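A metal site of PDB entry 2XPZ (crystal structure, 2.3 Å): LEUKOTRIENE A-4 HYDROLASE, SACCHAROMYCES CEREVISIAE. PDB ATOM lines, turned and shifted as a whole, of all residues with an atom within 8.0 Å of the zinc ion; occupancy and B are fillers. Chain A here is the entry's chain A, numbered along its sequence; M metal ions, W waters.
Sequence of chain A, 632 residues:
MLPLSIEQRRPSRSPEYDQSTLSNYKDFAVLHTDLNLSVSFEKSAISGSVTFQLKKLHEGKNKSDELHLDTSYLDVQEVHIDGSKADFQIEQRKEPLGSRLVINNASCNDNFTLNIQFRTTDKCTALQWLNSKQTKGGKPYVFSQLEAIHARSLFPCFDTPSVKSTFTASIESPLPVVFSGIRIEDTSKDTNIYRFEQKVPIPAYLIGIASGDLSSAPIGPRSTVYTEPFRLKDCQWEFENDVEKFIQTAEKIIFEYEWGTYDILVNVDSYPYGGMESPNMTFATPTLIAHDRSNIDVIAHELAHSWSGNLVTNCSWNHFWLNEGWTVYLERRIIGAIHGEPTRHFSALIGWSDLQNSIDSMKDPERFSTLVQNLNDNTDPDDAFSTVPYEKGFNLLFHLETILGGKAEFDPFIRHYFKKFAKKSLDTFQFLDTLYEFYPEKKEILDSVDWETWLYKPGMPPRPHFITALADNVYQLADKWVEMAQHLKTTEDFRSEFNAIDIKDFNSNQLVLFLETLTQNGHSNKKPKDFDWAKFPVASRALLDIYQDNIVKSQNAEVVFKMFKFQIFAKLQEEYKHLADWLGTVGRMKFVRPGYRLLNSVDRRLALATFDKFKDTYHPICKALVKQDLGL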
ATOM      1  N   GLU A 147      25.513 -11.852  18.847  1.00  0.00           N
ATOM      2  CA  GLU A 147      24.524 -12.493  19.716  1.00  0.00           C
ATOM      3  C   GLU A 147      25.178 -13.573  20.591  1.00  0.00           C
ATOM      4  O   GLU A 147      25.981 -14.368  20.096  1.00  0.00           O
ATOM      5  CB  GLU A 147      23.428 -13.111  18.843  1.00  0.00           C
ATOM      6  CG  GLU A 147      22.126 -13.435  19.568  1.00  0.00           C
ATOM      7  CD  GLU A 147      20.992 -13.831  18.643  1.00  0.00           C
ATOM      8  OE1 GLU A 147      21.219 -14.580  17.685  1.00  0.00           O
ATOM      9  OE2 GLU A 147      19.866 -13.377  18.874  1.00  0.00           O
ATOM     10  N   GLY A 275      24.177 -18.768   9.879  1.00  0.00           N
ATOM     11  CA  GLY A 275      23.492 -17.556   9.470  1.00  0.00           C
ATOM     12  C   GLY A 275      23.203 -16.585  10.599  1.00  0.00           C
ATOM     13  O   GLY A 275      23.253 -16.927  11.782  1.00  0.00           O
ATOM     14  N   MET A 276      22.899 -15.344  10.222  1.00  0.00           N
ATOM     15  CA  MET A 276      22.691 -14.281  11.180  1.00  0.00           C
ATOM     16  C   MET A 276      21.838 -13.221  10.499  1.00  0.00           C
ATOM     17  O   MET A 276      21.923 -13.044   9.299  1.00  0.00           O
ATOM     18  CB  MET A 276      24.017 -13.693  11.655  1.00  0.00           C
ATOM     19  CG  MET A 276      23.875 -12.631  12.714  1.00  0.00           C
ATOM     20  SD  MET A 276      22.926 -13.206  14.137  1.00  0.00           S
ATOM     21  CE  MET A 276      22.226 -11.656  14.721  1.00  0.00           C
ATOM     22  N   GLU A 277      21.001 -12.544  11.281  1.00  0.00           N
ATOM     23  CA  GLU A 277      19.970 -11.656  10.752  1.00  0.00           C
ATOM     24  C   GLU A 277      20.257 -10.197  11.078  1.00  0.00           C
ATOM     25  O   GLU A 277      19.350  -9.441  11.468  1.00  0.00           O
ATOM     26  CB  GLU A 277      18.600 -12.027  11.324  1.00  0.00           C
ATOM     27  CG  GLU A 277      18.423 -11.669  12.784  1.00  0.00           C
ATOM     28  CD  GLU A 277      19.087 -12.642  13.744  1.00  0.00           C
ATOM     29  OE1 GLU A 277      19.709 -13.620  13.289  1.00  0.00           O
ATOM     30  OE2 GLU A 277      18.975 -12.438  14.971  1.00  0.00           O
ATOM     31  N   HIS A 301      13.727 -17.092   6.933  1.00  0.00           N
ATOM     32  CA  HIS A 301      13.910 -16.949   8.371  1.00  0.00           C
ATOM     33  C   HIS A 301      14.599 -15.653   8.769  1.00  0.00           C
ATOM     34  O   HIS A 301      14.115 -14.906   9.598  1.00  0.00           O
ATOM     35  CB  HIS A 301      14.716 -18.128   8.894  1.00  0.00           C
ATOM     36  CG  HIS A 301      14.890 -18.102  10.373  1.00  0.00           C
ATOM     37  ND1 HIS A 301      13.979 -18.644  11.238  1.00  0.00           N
ATOM     38  CD2 HIS A 301      15.873 -17.574  11.142  1.00  0.00           C
ATOM     39  CE1 HIS A 301      14.389 -18.471  12.484  1.00  0.00           C
ATOM     40  NE2 HIS A 301      15.532 -17.826  12.445  1.00  0.00           N
ATOM     41  N   GLU A 302      15.758 -15.404   8.160  1.00  0.00           N
ATOM     42  CA  GLU A 302      16.509 -14.177   8.348  1.00  0.00           C
ATOM     43  C   GLU A 302      15.688 -12.998   7.897  1.00  0.00           C
ATOM     44  O   GLU A 302      15.674 -11.969   8.541  1.00  0.00           O
ATOM     45  CB  GLU A 302      17.807 -14.241   7.559  1.00  0.00           C
ATOM     46  CG  GLU A 302      19.000 -14.681   8.394  1.00  0.00           C
ATOM     47  CD  GLU A 302      19.009 -16.168   8.659  1.00  0.00           C
ATOM     48  OE1 GLU A 302      18.549 -16.920   7.782  1.00  0.00           O
ATOM     49  OE2 GLU A 302      19.495 -16.585   9.743  1.00  0.00           O
ATOM     50  N   ALA A 304      12.499 -12.868   7.829  1.00  0.00           N
ATOM     51  CA  ALA A 304      11.407 -12.733   8.783  1.00  0.00           C
ATOM     52  C   ALA A 304      11.837 -11.900   9.974  1.00  0.00           C
ATOM     53  O   ALA A 304      11.032 -11.176  10.553  1.00  0.00           O
ATOM     54  CB  ALA A 304      10.930 -14.102   9.229  1.00  0.00           C
ATOM     55  N   HIS A 305      13.109 -11.998  10.343  1.00  0.00           N
ATOM     56  CA  HIS A 305      13.635 -11.283  11.492  1.00  0.00           C
ATOM     57  C   HIS A 305      13.547  -9.786  11.333  1.00  0.00           C
ATOM     58  O   HIS A 305      13.639  -9.036  12.306  1.00  0.00           O
ATOM     59  CB  HIS A 305      15.094 -11.638  11.700  1.00  0.00           C
ATOM     60  CG  HIS A 305      15.292 -12.755  12.698  1.00  0.00           C
ATOM     61  ND1 HIS A 305      14.846 -12.656  13.969  1.00  0.00           N
ATOM     62  CD2 HIS A 305      15.918 -13.941  12.546  1.00  0.00           C
ATOM     63  CE1 HIS A 305      15.177 -13.792  14.620  1.00  0.00           C
ATOM     64  NE2 HIS A 305      15.810 -14.561  13.790  1.00  0.00           N
ATOM     65  N   SER A 308      10.278  -9.523  13.336  1.00  0.00           N
ATOM     66  CA  SER A 308      10.348 -10.058  14.695  1.00  0.00           C
ATOM     67  C   SER A 308      11.776 -10.286  15.167  1.00  0.00           C
ATOM     68  O   SER A 308      12.455 -11.186  14.688  1.00  0.00           O
ATOM     69  CB  SER A 308       9.581 -11.366  14.787  1.00  0.00           C
ATOM     70  OG  SER A 308      10.147 -12.321  13.919  1.00  0.00           O
ATOM     71  N   ASN A 310      14.232  -7.909  14.999  1.00  0.00           N
ATOM     72  CA  ASN A 310      14.966  -6.772  14.548  1.00  0.00           C
ATOM     73  C   ASN A 310      14.116  -5.562  14.753  1.00  0.00           C
ATOM     74  O   ASN A 310      14.553  -4.574  15.336  1.00  0.00           O
ATOM     75  CB  ASN A 310      15.358  -6.919  13.074  1.00  0.00           C
ATOM     76  CG  ASN A 310      16.373  -8.016  12.851  1.00  0.00           C
ATOM     77  OD1 ASN A 310      16.660  -8.824  13.739  1.00  0.00           O
ATOM     78  ND2 ASN A 310      16.927  -8.064  11.662  1.00  0.00           N
ATOM     79  N   PHE A 320      13.605 -14.601  24.969  1.00  0.00           N
ATOM     80  CA  PHE A 320      14.150 -14.806  23.657  1.00  0.00           C
ATOM     81  C   PHE A 320      13.167 -15.468  22.699  1.00  0.00           C
ATOM     82  O   PHE A 320      13.303 -15.330  21.484  1.00  0.00           O
ATOM     83  CB  PHE A 320      15.421 -15.642  23.784  1.00  0.00           C
ATOM     84  CG  PHE A 320      16.151 -15.821  22.506  1.00  0.00           C
ATOM     85  CD1 PHE A 320      16.440 -14.738  21.701  1.00  0.00           C
ATOM     86  CD2 PHE A 320      16.558 -17.077  22.104  1.00  0.00           C
ATOM     87  CE1 PHE A 320      17.120 -14.898  20.531  1.00  0.00           C
ATOM     88  CE2 PHE A 320      17.242 -17.238  20.925  1.00  0.00           C
ATOM     89  CZ  PHE A 320      17.530 -16.156  20.143  1.00  0.00           C
ATOM     90  N   ASN A 323      11.617 -13.445  20.065  1.00  0.00           N
ATOM     91  CA  ASN A 323      12.502 -13.184  18.968  1.00  0.00           C
ATOM     92  C   ASN A 323      12.343 -14.326  18.000  1.00  0.00           C
ATOM     93  O   ASN A 323      11.766 -14.176  16.930  1.00  0.00           O
ATOM     94  CB  ASN A 323      13.949 -13.124  19.488  1.00  0.00           C
ATOM     95  CG  ASN A 323      14.889 -12.373  18.549  1.00  0.00           C
ATOM     96  OD1 ASN A 323      14.692 -12.328  17.344  1.00  0.00           O
ATOM     97  ND2 ASN A 323      15.932 -11.786  19.118  1.00  0.00           N
ATOM     98  N   GLU A 324      12.796 -15.497  18.423  1.00  0.00           N
ATOM     99  CA  GLU A 324      12.951 -16.677  17.562  1.00  0.00           C
ATOM    100  C   GLU A 324      11.698 -17.497  17.248  1.00  0.00           C
ATOM    101  O   GLU A 324      11.570 -18.021  16.156  1.00  0.00           O
ATOM    102  CB  GLU A 324      14.022 -17.584  18.135  1.00  0.00           C
ATOM    103  CG  GLU A 324      15.402 -17.068  17.834  1.00  0.00           C
ATOM    104  CD  GLU A 324      15.628 -16.961  16.342  1.00  0.00           C
ATOM    105  OE1 GLU A 324      14.731 -17.370  15.571  1.00  0.00           O
ATOM    106  OE2 GLU A 324      16.701 -16.464  15.945  1.00  0.00           O
ATOM    107  N   GLY A 325      10.798 -17.604  18.221  1.00  0.00           N
ATOM    108  CA  GLY A 325       9.540 -18.291  17.993  1.00  0.00           C
ATOM    109  C   GLY A 325       8.674 -17.572  16.991  1.00  0.00           C
ATOM    110  O   GLY A 325       8.140 -18.188  16.086  1.00  0.00           O
ATOM    111  N   THR A 327       9.623 -15.790  14.786  1.00  0.00           N
ATOM    112  CA  THR A 327      10.319 -15.776  13.517  1.00  0.00           C
ATOM    113  C   THR A 327      10.152 -17.095  12.788  1.00  0.00           C
ATOM    114  O   THR A 327       9.974 -17.131  11.577  1.00  0.00           O
ATOM    115  CB  THR A 327      11.809 -15.500  13.700  1.00  0.00           C
ATOM    116  OG1 THR A 327      12.006 -14.141  14.069  1.00  0.00           O
ATOM    117  CG2 THR A 327      12.525 -15.759  12.411  1.00  0.00           C
ATOM    118  N   VAL A 328      10.223 -18.186  13.527  1.00  0.00           N
ATOM    119  CA  VAL A 328       9.926 -19.481  12.944  1.00  0.00           C
ATOM    120  C   VAL A 328       8.479 -19.501  12.453  1.00  0.00           C
ATOM    121  O   VAL A 328       8.210 -19.994  11.355  1.00  0.00           O
ATOM    122  CB  VAL A 328      10.182 -20.607  13.938  1.00  0.00           C
ATOM    123  CG1 VAL A 328       9.518 -21.863  13.458  1.00  0.00           C
ATOM    124  CG2 VAL A 328      11.679 -20.834  14.107  1.00  0.00           C
ATOM    125  N   GLU A 331       8.211 -17.320   9.494  1.00  0.00           N
ATOM    126  CA  GLU A 331       9.022 -18.010   8.487  1.00  0.00           C
ATOM    127  C   GLU A 331       8.235 -19.109   7.818  1.00  0.00           C
ATOM    128  O   GLU A 331       8.201 -19.218   6.597  1.00  0.00           O
ATOM    129  CB  GLU A 331      10.274 -18.615   9.133  1.00  0.00           C
ATOM    130  CG  GLU A 331      10.950 -19.698   8.299  1.00  0.00           C
ATOM    131  CD  GLU A 331      12.021 -20.431   9.091  1.00  0.00           C
ATOM    132  OE1 GLU A 331      12.144 -20.182  10.298  1.00  0.00           O
ATOM    133  OE2 GLU A 331      12.748 -21.266   8.506  1.00  0.00           O
ATOM    134  N   TYR A 390      12.751 -21.427  19.450  1.00  0.00           N
ATOM    135  CA  TYR A 390      12.278 -21.567  18.079  1.00  0.00           C
ATOM    136  C   TYR A 390      10.993 -22.381  17.962  1.00  0.00           C
ATOM    137  O   TYR A 390       9.983 -21.906  17.440  1.00  0.00           O
ATOM    138  CB  TYR A 390      13.363 -22.233  17.252  1.00  0.00           C
ATOM    139  CG  TYR A 390      14.687 -21.499  17.262  1.00  0.00           C
ATOM    140  CD1 TYR A 390      15.525 -21.575  18.355  1.00  0.00           C
ATOM    141  CD2 TYR A 390      15.086 -20.730  16.173  1.00  0.00           C
ATOM    142  CE1 TYR A 390      16.742 -20.909  18.374  1.00  0.00           C
ATOM    143  CE2 TYR A 390      16.300 -20.062  16.178  1.00  0.00           C
ATOM    144  CZ  TYR A 390      17.126 -20.156  17.278  1.00  0.00           C
ATOM    145  OH  TYR A 390      18.345 -19.500  17.288  1.00  0.00           O
HETATM  146 ZN    ZN M   1      16.741 -16.684  13.817  1.00  0.00          ZN
HETATM  147  O   HOH W   1      19.497 -16.728  12.321  1.00  0.00           O
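A ring nitrogen (ND1) of His 301 is in hydrogen-bond range of the side-chain carboxylate of Glu 331 (2.6 Å).
A ring nitrogen (ND1) of His 305 lies within hydrogen-bond range of the side-chain hydroxyl of Thr 327, 3.2 Å away.
The backbone carbonyl oxygen (O) of His 305 lies close to the backbone NH (N) of Asn 310 (3.0 Å).
The side-chain amide oxygen (OD1) of Asn 323 lies close to a ring nitrogen (ND1) of His 305, at 3.4 Å.
The backbone carbonyl oxygen (O) of Ser 308 lies within hydrogen-bond range of a ring nitrogen (ND1) of His 305.
The nearest printed residue that does not touch the zinc ion is Tyr 390 (4.1 Å).
The zinc ion is bound by OE2 of Glu 324 (2.1 Å), NE2 of His 301 (2.2 Å) and NE2 of His 305 (2.3 Å).
The zinc ion has three donor atoms within binding distance.
Slightly farther from the zinc ion lies OE1 of Glu 324 (2.8 Å).
Water W1 bridges OE2 of Glu 302 (2.6 Å) and OE1 of Glu 277 (3.3 Å).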
